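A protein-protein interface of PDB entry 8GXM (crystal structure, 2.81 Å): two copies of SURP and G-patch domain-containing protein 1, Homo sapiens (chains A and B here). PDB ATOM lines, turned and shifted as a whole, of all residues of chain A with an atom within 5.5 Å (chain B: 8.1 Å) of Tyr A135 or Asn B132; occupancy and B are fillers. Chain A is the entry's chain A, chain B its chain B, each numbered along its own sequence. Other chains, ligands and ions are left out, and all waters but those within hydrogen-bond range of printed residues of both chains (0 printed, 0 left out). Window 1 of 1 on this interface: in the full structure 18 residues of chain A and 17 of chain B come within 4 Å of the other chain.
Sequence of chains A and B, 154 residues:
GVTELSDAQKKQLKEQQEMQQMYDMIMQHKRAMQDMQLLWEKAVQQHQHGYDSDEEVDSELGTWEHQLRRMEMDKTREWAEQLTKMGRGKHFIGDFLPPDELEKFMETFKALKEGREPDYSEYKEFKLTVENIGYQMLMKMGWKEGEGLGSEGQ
The side-chain amide nitrogen of Asn B132 lies close to the side-chain amide oxygen of Asn A132, 2.4 Å away. OE1 of Glu A131 lies close to OD1 of Asn B132 (3.3 Å). The side-chain hydroxyl of Tyr A135 is in hydrogen-bond range of the side-chain amide nitrogen of Gln B136 (3.1 Å). The backbone carbonyl oxygen (O) of Leu B128 lies within hydrogen-bond range of the side-chain amide nitrogen (ND2) of Asn A132 (3.3 Å).
Printed residues of chain B that touch a printed residue of chain A: Leu B128, Thr B129, Glu B131, Asn B132, Tyr B135, Gln B136, Leu B138 and Met B139. Along chain B the printed residues that touch a printed residue of chain A span positions 128 to 139. Hydrophobic or aromatic side chains of chain A that line the printed part of chain B: Leu A128, Tyr A135, Leu A138 and Met A139. Among the printed residues, 16 pairs touch across the chains. Among the printed residues, no Asp or Glu carboxylate lies within 4 Å of a Lys or Arg side-chain nitrogen of the other chain.
Tyr A135 touches just these residues of chain B: Asn B132, Tyr B135, Gln B136 and Met B139. Of chain A, only Leu A128, Glu A131, Asn A132 and Tyr A135 come within 4 Å of Asn B132. Of the printed residues of chain A, Leu B138 touches Met A139. Of the printed residues of chain A, Leu B128 touches Leu A128 and Asn A132. Printed residues of chain A within 4 Å of Met B139: Tyr A135 and Leu A138. Printed residues of chain A within 4 Å of Gln B136: Lys A30 (3.5 Å), Glu A131 (3.7 Å) and Tyr A135 (3.1 Å). Of the printed residues of chain A, Glu B131 touches Asn A132. The nearest printed residue of chain A that does not touch Asn B132 is Val A130 (6.3 Å).
Leu B128 touches its own counterpart, Leu A128. Leu A128 touches Asn B132, and with the chains exchanged Asn A132 touches Leu B128. Tyr A135 touches Asn B132, but with the chains exchanged Asn A132 does not touch Tyr B135 (4.02 Å). Tyr B135 touches its own counterpart, Tyr A135. 12 positions are printed for both chains.
The backbone carbonyl oxygen (O) of Glu B125 sits at hydrogen-bond distance from the side-chain hydroxyl (OG1) of Thr B129 (2.5 Å). The side-chain carboxylate (OE1) of Glu A131 is in hydrogen-bond range of the side-chain hydroxyl (OH) of Tyr A135. OE2 of Glu B131 sits at hydrogen-bond distance from NE2 of His B29, at 3.2 Å. The backbone carbonyl oxygen (O) of Leu A128 lies close to the side-chain amide oxygen (OD1) of Asn A132 (3.5 Å). The side-chain amide oxygen (OD1) of Asn B132 lies within hydrogen-bond range of the side-chain amide nitrogen (NE2) of Gln B136 (2.7 Å).
NZ of Lys A30 touches CG of Gln B136, at 3.5 Å. Leu A128 touches Thr B129 (CD1 to OG1, 3.8 Å). OE1 of Glu A131 touches NE2 of Gln B136 (3.7 Å). Glu B131 touches Asn A132. Asn B132 touches Tyr A135 (ND2 to CE2, 3.6 Å). Tyr B135 touches Tyr A135. Met B139 touches Tyr A135 (SD to CE1, 3.7 Å). CG of Gln A136 touches OH of Tyr B135, at 3.0 Å. Leu A138 touches Met B139 (CD2 to CE, 3.4 Å). CD2 of Leu B138 touches SD of Met A139, at 3.6 Å.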
ATOM      1  N   ILE A  26      28.636 -29.186  23.290  1.00  0.00           N
ATOM      2  CA  ILE A  26      27.287 -28.678  23.505  1.00  0.00           C
ATOM      3  C   ILE A  26      26.927 -28.745  24.987  1.00  0.00           C
ATOM      4  O   ILE A  26      26.520 -27.744  25.587  1.00  0.00           O
ATOM      5  CB  ILE A  26      26.292 -29.463  22.629  1.00  0.00           C
ATOM      6  CG1 ILE A  26      26.290 -28.943  21.195  1.00  0.00           C
ATOM      7  CG2 ILE A  26      24.885 -29.424  23.203  1.00  0.00           C
ATOM      8  CD1 ILE A  26      25.466 -29.838  20.238  1.00  0.00           C
ATOM      9  N   LYS A  30      25.876 -25.998  27.475  1.00  0.00           N
ATOM     10  CA  LYS A  30      24.568 -26.151  28.087  1.00  0.00           C
ATOM     11  C   LYS A  30      24.642 -25.952  29.596  1.00  0.00           C
ATOM     12  O   LYS A  30      23.819 -25.233  30.185  1.00  0.00           O
ATOM     13  CB  LYS A  30      24.007 -27.516  27.745  1.00  0.00           C
ATOM     14  CG  LYS A  30      22.530 -27.663  28.008  1.00  0.00           C
ATOM     15  CD  LYS A  30      21.853 -28.501  26.914  1.00  0.00           C
ATOM     16  CE  LYS A  30      20.661 -29.299  27.465  1.00  0.00           C
ATOM     17  NZ  LYS A  30      20.570 -30.704  26.914  1.00  0.00           N
ATOM     18  N   LEU A 128      18.305 -18.790  21.293  1.00  0.00           N
ATOM     19  CA  LEU A 128      17.633 -20.012  20.868  1.00  0.00           C
ATOM     20  C   LEU A 128      18.104 -20.450  19.488  1.00  0.00           C
ATOM     21  O   LEU A 128      18.299 -21.644  19.247  1.00  0.00           O
ATOM     22  CB  LEU A 128      16.126 -19.806  20.896  1.00  0.00           C
ATOM     23  CG  LEU A 128      15.606 -19.818  22.344  1.00  0.00           C
ATOM     24  CD1 LEU A 128      14.253 -19.196  22.448  1.00  0.00           C
ATOM     25  CD2 LEU A 128      15.556 -21.243  22.863  1.00  0.00           C
ATOM     26  N   VAL A 130      21.083 -19.973  17.830  1.00  0.00           N
ATOM     27  CA  VAL A 130      22.398 -20.625  17.864  1.00  0.00           C
ATOM     28  C   VAL A 130      22.303 -21.978  18.567  1.00  0.00           C
ATOM     29  O   VAL A 130      22.905 -22.964  18.130  1.00  0.00           O
ATOM     30  CB  VAL A 130      23.473 -19.710  18.502  1.00  0.00           C
ATOM     31  CG1 VAL A 130      23.347 -18.288  17.985  1.00  0.00           C
ATOM     32  CG2 VAL A 130      23.390 -19.686  19.964  1.00  0.00           C
ATOM     33  N   GLU A 131      21.517 -22.059  19.637  1.00  0.00           N
ATOM     34  CA  GLU A 131      21.319 -23.346  20.272  1.00  0.00           C
ATOM     35  C   GLU A 131      20.795 -24.363  19.265  1.00  0.00           C
ATOM     36  O   GLU A 131      21.291 -25.487  19.187  1.00  0.00           O
ATOM     37  CB  GLU A 131      20.357 -23.185  21.437  1.00  0.00           C
ATOM     38  CG  GLU A 131      20.965 -23.185  22.806  1.00  0.00           C
ATOM     39  CD  GLU A 131      19.947 -23.710  23.816  1.00  0.00           C
ATOM     40  OE1 GLU A 131      19.889 -24.967  24.053  1.00  0.00           O
ATOM     41  OE2 GLU A 131      19.173 -22.859  24.341  1.00  0.00           O
ATOM     42  N   ASN A 132      19.795 -23.985  18.474  1.00  0.00           N
ATOM     43  CA  ASN A 132      19.256 -24.939  17.520  1.00  0.00           C
ATOM     44  C   ASN A 132      20.263 -25.229  16.420  1.00  0.00           C
ATOM     45  O   ASN A 132      20.311 -26.344  15.896  1.00  0.00           O
ATOM     46  CB  ASN A 132      17.943 -24.417  16.931  1.00  0.00           C
ATOM     47  CG  ASN A 132      16.780 -24.454  17.945  1.00  0.00           C
ATOM     48  OD1 ASN A 132      16.939 -24.826  19.128  1.00  0.00           O
ATOM     49  ND2 ASN A 132      15.593 -24.042  17.477  1.00  0.00           N
ATOM     50  N   ILE A 133      21.090 -24.253  16.065  1.00  0.00           N
ATOM     51  CA  ILE A 133      22.065 -24.520  15.019  1.00  0.00           C
ATOM     52  C   ILE A 133      23.052 -25.579  15.479  1.00  0.00           C
ATOM     53  O   ILE A 133      23.379 -26.511  14.729  1.00  0.00           O
ATOM     54  CB  ILE A 133      22.773 -23.226  14.597  1.00  0.00           C
ATOM     55  CG1 ILE A 133      21.863 -22.423  13.665  1.00  0.00           C
ATOM     56  CG2 ILE A 133      24.095 -23.566  13.935  1.00  0.00           C
ATOM     57  CD1 ILE A 133      22.273 -20.977  13.507  1.00  0.00           C
ATOM     58  N   GLY A 134      23.513 -25.479  16.730  1.00  0.00           N
ATOM     59  CA  GLY A 134      24.419 -26.486  17.259  1.00  0.00           C
ATOM     60  C   GLY A 134      23.780 -27.855  17.326  1.00  0.00           C
ATOM     61  O   GLY A 134      24.430 -28.864  17.056  1.00  0.00           O
ATOM     62  N   TYR A 135      22.493 -27.912  17.687  1.00  0.00           N
ATOM     63  CA  TYR A 135      21.807 -29.200  17.728  1.00  0.00           C
ATOM     64  C   TYR A 135      21.741 -29.808  16.343  1.00  0.00           C
ATOM     65  O   TYR A 135      21.931 -31.020  16.183  1.00  0.00           O
ATOM     66  CB  TYR A 135      20.404 -29.037  18.310  1.00  0.00           C
ATOM     67  CG  TYR A 135      20.411 -28.820  19.810  1.00  0.00           C
ATOM     68  CD1 TYR A 135      21.143 -29.656  20.649  1.00  0.00           C
ATOM     69  CD2 TYR A 135      19.695 -27.783  20.393  1.00  0.00           C
ATOM     70  CE1 TYR A 135      21.159 -29.468  22.016  1.00  0.00           C
ATOM     71  CE2 TYR A 135      19.711 -27.591  21.763  1.00  0.00           C
ATOM     72  CZ  TYR A 135      20.442 -28.433  22.563  1.00  0.00           C
ATOM     73  OH  TYR A 135      20.453 -28.233  23.920  1.00  0.00           O
ATOM     74  N   GLN A 136      21.529 -28.955  15.326  1.00  0.00           N
ATOM     75  CA  GLN A 136      21.344 -29.401  13.948  1.00  0.00           C
ATOM     76  C   GLN A 136      22.613 -30.034  13.389  1.00  0.00           C
ATOM     77  O   GLN A 136      22.570 -31.127  12.797  1.00  0.00           O
ATOM     78  CB  GLN A 136      20.923 -28.223  13.082  1.00  0.00           C
ATOM     79  CG  GLN A 136      19.463 -27.828  13.229  1.00  0.00           C
ATOM     80  CD  GLN A 136      19.044 -26.801  12.195  1.00  0.00           C
ATOM     81  OE1 GLN A 136      19.201 -27.014  10.994  1.00  0.00           O
ATOM     82  NE2 GLN A 136      18.531 -25.669  12.657  1.00  0.00           N
ATOM     83  N   MET A 137      23.762 -29.371  13.559  1.00  0.00           N
ATOM     84  CA  MET A 137      24.965 -29.973  13.003  1.00  0.00           C
ATOM     85  C   MET A 137      25.374 -31.240  13.742  1.00  0.00           C
ATOM     86  O   MET A 137      25.873 -32.169  13.101  1.00  0.00           O
ATOM     87  CB  MET A 137      26.114 -28.980  12.965  1.00  0.00           C
ATOM     88  CG  MET A 137      26.064 -27.895  13.957  1.00  0.00           C
ATOM     89  SD  MET A 137      27.421 -26.798  13.529  1.00  0.00           S
ATOM     90  CE  MET A 137      26.650 -25.683  12.365  1.00  0.00           C
ATOM     91  N   LEU A 138      25.170 -31.325  15.068  1.00  0.00           N
ATOM     92  CA  LEU A 138      25.409 -32.615  15.720  1.00  0.00           C
ATOM     93  C   LEU A 138      24.559 -33.696  15.088  1.00  0.00           C
ATOM     94  O   LEU A 138      24.922 -34.873  15.117  1.00  0.00           O
ATOM     95  CB  LEU A 138      25.132 -32.568  17.222  1.00  0.00           C
ATOM     96  CG  LEU A 138      25.118 -33.948  17.935  1.00  0.00           C
ATOM     97  CD1 LEU A 138      26.509 -34.530  18.189  1.00  0.00           C
ATOM     98  CD2 LEU A 138      24.328 -33.939  19.217  1.00  0.00           C
ATOM     99  N   MET A 139      23.444 -33.317  14.475  1.00  0.00           N
ATOM    100  CA  MET A 139      22.607 -34.341  13.869  1.00  0.00           C
ATOM    101  C   MET A 139      23.152 -34.802  12.527  1.00  0.00           C
ATOM    102  O   MET A 139      23.196 -36.008  12.265  1.00  0.00           O
ATOM    103  CB  MET A 139      21.187 -33.822  13.705  1.00  0.00           C
ATOM    104  CG  MET A 139      20.407 -33.869  14.973  1.00  0.00           C
ATOM    105  SD  MET A 139      18.684 -34.096  14.502  1.00  0.00           S
ATOM    106  CE  MET A 139      18.613 -33.324  12.912  1.00  0.00           C
ATOM    107  N   ILE B  26      11.168 -34.891  13.782  1.00  0.00           N
ATOM    108  CA  ILE B  26      12.006 -33.714  13.598  1.00  0.00           C
ATOM    109  C   ILE B  26      12.142 -33.392  12.117  1.00  0.00           C
ATOM    110  O   ILE B  26      12.013 -32.231  11.708  1.00  0.00           O
ATOM    111  CB  ILE B  26      13.368 -33.933  14.278  1.00  0.00           C
ATOM    112  CG1 ILE B  26      13.185 -33.934  15.785  1.00  0.00           C
ATOM    113  CG2 ILE B  26      14.375 -32.855  13.899  1.00  0.00           C
ATOM    114  CD1 ILE B  26      14.487 -33.849  16.531  1.00  0.00           C
ATOM    115  N   HIS B  29       8.740 -32.150  10.676  1.00  0.00           N
ATOM    116  CA  HIS B  29       8.505 -30.762  11.066  1.00  0.00           C
ATOM    117  C   HIS B  29       9.436 -29.837  10.311  1.00  0.00           C
ATOM    118  O   HIS B  29       8.999 -28.849   9.710  1.00  0.00           O
ATOM    119  CB  HIS B  29       8.691 -30.577  12.565  1.00  0.00           C
ATOM    120  CG  HIS B  29       8.648 -29.147  13.009  1.00  0.00           C
ATOM    121  ND1 HIS B  29       7.505 -28.378  12.939  1.00  0.00           N
ATOM    122  CD2 HIS B  29       9.604 -28.350  13.555  1.00  0.00           C
ATOM    123  CE1 HIS B  29       7.758 -27.173  13.427  1.00  0.00           C
ATOM    124  NE2 HIS B  29       9.024 -27.129  13.805  1.00  0.00           N
ATOM    125  N   TRP B  79       3.017 -29.826  16.014  1.00  0.00           N
ATOM    126  CA  TRP B  79       4.368 -30.279  16.327  1.00  0.00           C
ATOM    127  C   TRP B  79       4.566 -30.337  17.835  1.00  0.00           C
ATOM    128  O   TRP B  79       5.004 -31.361  18.382  1.00  0.00           O
ATOM    129  CB  TRP B  79       5.385 -29.353  15.665  1.00  0.00           C
ATOM    130  CG  TRP B  79       6.839 -29.600  15.989  1.00  0.00           C
ATOM    131  CD1 TRP B  79       7.784 -28.641  16.241  1.00  0.00           C
ATOM    132  CD2 TRP B  79       7.523 -30.862  16.056  1.00  0.00           C
ATOM    133  NE1 TRP B  79       9.007 -29.234  16.482  1.00  0.00           N
ATOM    134  CE2 TRP B  79       8.874 -30.592  16.369  1.00  0.00           C
ATOM    135  CE3 TRP B  79       7.132 -32.189  15.867  1.00  0.00           C
ATOM    136  CZ2 TRP B  79       9.829 -31.596  16.507  1.00  0.00           C
ATOM    137  CZ3 TRP B  79       8.090 -33.195  16.011  1.00  0.00           C
ATOM    138  CH2 TRP B  79       9.420 -32.889  16.322  1.00  0.00           C
ATOM    139  N   LEU B  83       5.115 -33.526  20.454  1.00  0.00           N
ATOM    140  CA  LEU B  83       6.234 -33.609  21.390  1.00  0.00           C
ATOM    141  C   LEU B  83       5.786 -34.051  22.773  1.00  0.00           C
ATOM    142  O   LEU B  83       6.452 -34.873  23.416  1.00  0.00           O
ATOM    143  CB  LEU B  83       6.950 -32.262  21.485  1.00  0.00           C
ATOM    144  CG  LEU B  83       8.350 -32.290  20.905  1.00  0.00           C
ATOM    145  CD1 LEU B  83       8.256 -32.626  19.435  1.00  0.00           C
ATOM    146  CD2 LEU B  83       9.014 -30.963  21.102  1.00  0.00           C
ATOM    147  N   PHE B  96      13.034 -29.176  30.814  1.00  0.00           N
ATOM    148  CA  PHE B  96      13.871 -28.406  29.903  1.00  0.00           C
ATOM    149  C   PHE B  96      13.807 -26.900  30.098  1.00  0.00           C
ATOM    150  O   PHE B  96      14.600 -26.181  29.476  1.00  0.00           O
ATOM    151  CB  PHE B  96      13.479 -28.723  28.454  1.00  0.00           C
ATOM    152  CG  PHE B  96      13.436 -30.193  28.158  1.00  0.00           C
ATOM    153  CD1 PHE B  96      14.595 -30.878  27.837  1.00  0.00           C
ATOM    154  CD2 PHE B  96      12.244 -30.893  28.220  1.00  0.00           C
ATOM    155  CE1 PHE B  96      14.571 -32.232  27.570  1.00  0.00           C
ATOM    156  CE2 PHE B  96      12.209 -32.256  27.963  1.00  0.00           C
ATOM    157  CZ  PHE B  96      13.374 -32.926  27.629  1.00  0.00           C
ATOM    158  N   LEU B  97      12.896 -26.392  30.922  1.00  0.00           N
ATOM    159  CA  LEU B  97      12.753 -24.950  31.036  1.00  0.00           C
ATOM    160  C   LEU B  97      12.841 -24.499  32.487  1.00  0.00           C
ATOM    161  O   LEU B  97      12.372 -25.203  33.387  1.00  0.00           O
ATOM    162  CB  LEU B  97      11.416 -24.501  30.445  1.00  0.00           C
ATOM    163  CG  LEU B  97      11.240 -24.754  28.952  1.00  0.00           C
ATOM    164  CD1 LEU B  97       9.868 -24.309  28.486  1.00  0.00           C
ATOM    165  CD2 LEU B  97      12.333 -24.038  28.176  1.00  0.00           C
ATOM    166  N   GLU B 125       9.455 -17.022  19.737  1.00  0.00           N
ATOM    167  CA  GLU B 125      10.098 -17.617  20.900  1.00  0.00           C
ATOM    168  C   GLU B 125       9.628 -19.048  21.096  1.00  0.00           C
ATOM    169  O   GLU B 125      10.407 -19.915  21.509  1.00  0.00           O
ATOM    170  CB  GLU B 125       9.779 -16.787  22.141  1.00  0.00           C
ATOM    171  CG  GLU B 125      10.968 -16.373  23.022  1.00  0.00           C
ATOM    172  CD  GLU B 125      10.513 -15.885  24.418  1.00  0.00           C
ATOM    173  OE1 GLU B 125      10.750 -16.601  25.422  1.00  0.00           O
ATOM    174  OE2 GLU B 125       9.900 -14.790  24.501  1.00  0.00           O
ATOM    175  N   PHE B 126       8.361 -19.310  20.789  1.00  0.00           N
ATOM    176  CA  PHE B 126       7.759 -20.608  21.028  1.00  0.00           C
ATOM    177  C   PHE B 126       8.148 -21.617  19.945  1.00  0.00           C
ATOM    178  O   PHE B 126       8.497 -22.769  20.245  1.00  0.00           O
ATOM    179  CB  PHE B 126       6.256 -20.421  21.084  1.00  0.00           C
ATOM    180  CG  PHE B 126       5.503 -21.674  21.341  1.00  0.00           C
ATOM    181  CD1 PHE B 126       5.338 -22.147  22.633  1.00  0.00           C
ATOM    182  CD2 PHE B 126       4.929 -22.364  20.298  1.00  0.00           C
ATOM    183  CE1 PHE B 126       4.621 -23.286  22.880  1.00  0.00           C
ATOM    184  CE2 PHE B 126       4.221 -23.501  20.534  1.00  0.00           C
ATOM    185  CZ  PHE B 126       4.065 -23.967  21.834  1.00  0.00           C
ATOM    186  N   LYS B 127       8.076 -21.202  18.679  1.00  0.00           N
ATOM    187  CA  LYS B 127       8.539 -22.053  17.597  1.00  0.00           C
ATOM    188  C   LYS B 127       9.940 -22.578  17.888  1.00  0.00           C
ATOM    189  O   LYS B 127      10.209 -23.786  17.794  1.00  0.00           O
ATOM    190  CB  LYS B 127       8.523 -21.281  16.271  1.00  0.00           C
ATOM    191  CG  LYS B 127       8.653 -22.221  15.092  1.00  0.00           C
ATOM    192  CD  LYS B 127       9.529 -21.687  13.989  1.00  0.00           C
ATOM    193  CE  LYS B 127       8.822 -20.546  13.249  1.00  0.00           C
ATOM    194  NZ  LYS B 127       9.637 -19.957  12.116  1.00  0.00           N
ATOM    195  N   LEU B 128      10.844 -21.670  18.253  1.00  0.00           N
ATOM    196  CA  LEU B 128      12.232 -22.042  18.481  1.00  0.00           C
ATOM    197  C   LEU B 128      12.366 -22.946  19.690  1.00  0.00           C
ATOM    198  O   LEU B 128      13.304 -23.745  19.768  1.00  0.00           O
ATOM    199  CB  LEU B 128      13.070 -20.789  18.681  1.00  0.00           C
ATOM    200  CG  LEU B 128      13.422 -19.972  17.443  1.00  0.00           C
ATOM    201  CD1 LEU B 128      14.104 -18.659  17.842  1.00  0.00           C
ATOM    202  CD2 LEU B 128      14.332 -20.776  16.565  1.00  0.00           C
ATOM    203  N   THR B 129      11.441 -22.844  20.631  1.00  0.00           N
ATOM    204  CA  THR B 129      11.614 -23.550  21.888  1.00  0.00           C
ATOM    205  C   THR B 129      11.168 -24.995  21.756  1.00  0.00           C
ATOM    206  O   THR B 129      11.814 -25.893  22.310  1.00  0.00           O
ATOM    207  CB  THR B 129      10.841 -22.831  22.999  1.00  0.00           C
ATOM    208  OG1 THR B 129      11.386 -21.528  23.161  1.00  0.00           O
ATOM    209  CG2 THR B 129      10.971 -23.539  24.316  1.00  0.00           C
ATOM    210  N   VAL B 130      10.072 -25.248  21.037  1.00  0.00           N
ATOM    211  CA  VAL B 130       9.738 -26.630  20.720  1.00  0.00           C
ATOM    212  C   VAL B 130      10.835 -27.241  19.854  1.00  0.00           C
ATOM    213  O   VAL B 130      11.328 -28.336  20.153  1.00  0.00           O
ATOM    214  CB  VAL B 130       8.345 -26.738  20.073  1.00  0.00           C
ATOM    215  CG1 VAL B 130       7.361 -25.896  20.860  1.00  0.00           C
ATOM    216  CG2 VAL B 130       8.353 -26.304  18.655  1.00  0.00           C
ATOM    217  N   GLU B 131      11.281 -26.522  18.812  1.00  0.00           N
ATOM    218  CA  GLU B 131      12.396 -27.031  18.028  1.00  0.00           C
ATOM    219  C   GLU B 131      13.540 -27.409  18.964  1.00  0.00           C
ATOM    220  O   GLU B 131      14.043 -28.538  18.935  1.00  0.00           O
ATOM    221  CB  GLU B 131      12.839 -26.007  16.972  1.00  0.00           C
ATOM    222  CG  GLU B 131      12.129 -26.118  15.605  1.00  0.00           C
ATOM    223  CD  GLU B 131      11.900 -24.744  14.915  1.00  0.00           C
ATOM    224  OE1 GLU B 131      12.624 -23.770  15.254  1.00  0.00           O
ATOM    225  OE2 GLU B 131      10.995 -24.626  14.033  1.00  0.00           O
ATOM    226  N   ASN B 132      13.877 -26.506  19.881  1.00  0.00           N
ATOM    227  CA  ASN B 132      14.993 -26.722  20.794  1.00  0.00           C
ATOM    228  C   ASN B 132      14.766 -27.940  21.669  1.00  0.00           C
ATOM    229  O   ASN B 132      15.633 -28.812  21.782  1.00  0.00           O
ATOM    230  CB  ASN B 132      15.168 -25.489  21.662  1.00  0.00           C
ATOM    231  CG  ASN B 132      16.538 -25.377  22.240  1.00  0.00           C
ATOM    232  OD1 ASN B 132      16.763 -25.765  23.385  1.00  0.00           O
ATOM    233  ND2 ASN B 132      17.473 -24.804  21.467  1.00  0.00           N
ATOM    234  N   ILE B 133      13.614 -28.003  22.326  1.00  0.00           N
ATOM    235  CA  ILE B 133      13.303 -29.153  23.172  1.00  0.00           C
ATOM    236  C   ILE B 133      13.334 -30.450  22.358  1.00  0.00           C
ATOM    237  O   ILE B 133      13.872 -31.469  22.804  1.00  0.00           O
ATOM    238  CB  ILE B 133      11.944 -28.940  23.859  1.00  0.00           C
ATOM    239  CG1 ILE B 133      12.083 -27.873  24.939  1.00  0.00           C
ATOM    240  CG2 ILE B 133      11.438 -30.229  24.440  1.00  0.00           C
ATOM    241  CD1 ILE B 133      10.789 -27.199  25.325  1.00  0.00           C
ATOM    242  N   GLY B 134      12.764 -30.428  21.151  1.00  0.00           N
ATOM    243  CA  GLY B 134      12.822 -31.605  20.297  1.00  0.00           C
ATOM    244  C   GLY B 134      14.230 -32.135  20.138  1.00  0.00           C
ATOM    245  O   GLY B 134      14.496 -33.307  20.394  1.00  0.00           O
ATOM    246  N   TYR B 135      15.157 -31.271  19.725  1.00  0.00           N
ATOM    247  CA  TYR B 135      16.548 -31.671  19.581  1.00  0.00           C
ATOM    248  C   TYR B 135      17.108 -32.175  20.900  1.00  0.00           C
ATOM    249  O   TYR B 135      17.933 -33.099  20.930  1.00  0.00           O
ATOM    250  CB  TYR B 135      17.391 -30.496  19.109  1.00  0.00           C
ATOM    251  CG  TYR B 135      17.147 -29.984  17.710  1.00  0.00           C
ATOM    252  CD1 TYR B 135      17.292 -30.807  16.591  1.00  0.00           C
ATOM    253  CD2 TYR B 135      16.829 -28.647  17.496  1.00  0.00           C
ATOM    254  CE1 TYR B 135      17.088 -30.303  15.294  1.00  0.00           C
ATOM    255  CE2 TYR B 135      16.638 -28.153  16.227  1.00  0.00           C
ATOM    256  CZ  TYR B 135      16.766 -28.980  15.135  1.00  0.00           C
ATOM    257  OH  TYR B 135      16.566 -28.451  13.886  1.00  0.00           O
ATOM    258  N   GLN B 136      16.711 -31.555  22.007  1.00  0.00           N
ATOM    259  CA  GLN B 136      17.259 -31.988  23.285  1.00  0.00           C
ATOM    260  C   GLN B 136      16.765 -33.382  23.638  1.00  0.00           C
ATOM    261  O   GLN B 136      17.519 -34.194  24.195  1.00  0.00           O
ATOM    262  CB  GLN B 136      16.891 -31.006  24.382  1.00  0.00           C
ATOM    263  CG  GLN B 136      17.985 -30.047  24.712  1.00  0.00           C
ATOM    264  CD  GLN B 136      17.478 -28.904  25.558  1.00  0.00           C
ATOM    265  OE1 GLN B 136      16.938 -29.123  26.639  1.00  0.00           O
ATOM    266  NE2 GLN B 136      17.629 -27.669  25.060  1.00  0.00           N
ATOM    267  N   MET B 137      15.501 -33.675  23.311  1.00  0.00           N
ATOM    268  CA  MET B 137      14.942 -34.998  23.563  1.00  0.00           C
ATOM    269  C   MET B 137      15.649 -36.056  22.728  1.00  0.00           C
ATOM    270  O   MET B 137      16.090 -37.089  23.244  1.00  0.00           O
ATOM    271  CB  MET B 137      13.449 -34.985  23.261  1.00  0.00           C
ATOM    272  CG  MET B 137      12.623 -34.182  24.267  1.00  0.00           C
ATOM    273  SD  MET B 137      10.863 -34.323  23.909  1.00  0.00           S
ATOM    274  CE  MET B 137      10.849 -35.864  22.982  1.00  0.00           C
ATOM    275  N   LEU B 138      15.754 -35.818  21.433  1.00  0.00           N
ATOM    276  CA  LEU B 138      16.540 -36.696  20.586  1.00  0.00           C
ATOM    277  C   LEU B 138      17.910 -36.967  21.197  1.00  0.00           C
ATOM    278  O   LEU B 138      18.280 -38.117  21.455  1.00  0.00           O
ATOM    279  CB  LEU B 138      16.685 -36.068  19.200  1.00  0.00           C
ATOM    280  CG  LEU B 138      17.184 -37.093  18.204  1.00  0.00           C
ATOM    281  CD1 LEU B 138      16.176 -38.245  18.168  1.00  0.00           C
ATOM    282  CD2 LEU B 138      17.406 -36.469  16.829  1.00  0.00           C
ATOM    283  N   MET B 139      18.681 -35.913  21.446  1.00  0.00           N
ATOM    284  CA  MET B 139      20.059 -36.148  21.854  1.00  0.00           C
ATOM    285  C   MET B 139      20.137 -36.861  23.199  1.00  0.00           C
ATOM    286  O   MET B 139      21.163 -37.469  23.500  1.00  0.00           O
ATOM    287  CB  MET B 139      20.840 -34.831  21.889  1.00  0.00           C
ATOM    288  CG  MET B 139      20.766 -34.139  23.210  1.00  0.00           C
ATOM    289  SD  MET B 139      21.985 -32.808  23.373  1.00  0.00           S
ATOM    290  CE  MET B 139      23.306 -33.458  22.404  1.00  0.00           C
ATOM    291  N   LYS B 140      19.077 -36.824  24.004  1.00  0.00           N
ATOM    292  CA  LYS B 140      19.048 -37.569  25.253  1.00  0.00           C
ATOM    293  C   LYS B 140      18.627 -39.019  25.048  1.00  0.00           C
ATOM    294  O   LYS B 140      18.496 -39.758  26.025  1.00  0.00           O
ATOM    295  CB  LYS B 140      18.122 -36.868  26.266  1.00  0.00           C
ATOM    296  CG  LYS B 140      18.248 -37.348  27.725  1.00  0.00           C
ATOM    297  CD  LYS B 140      19.006 -36.381  28.656  1.00  0.00           C
ATOM    298  CE  LYS B 140      19.536 -37.120  29.920  1.00  0.00           C
ATOM    299  NZ  LYS B 140      19.712 -36.230  31.108  1.00  0.00           N
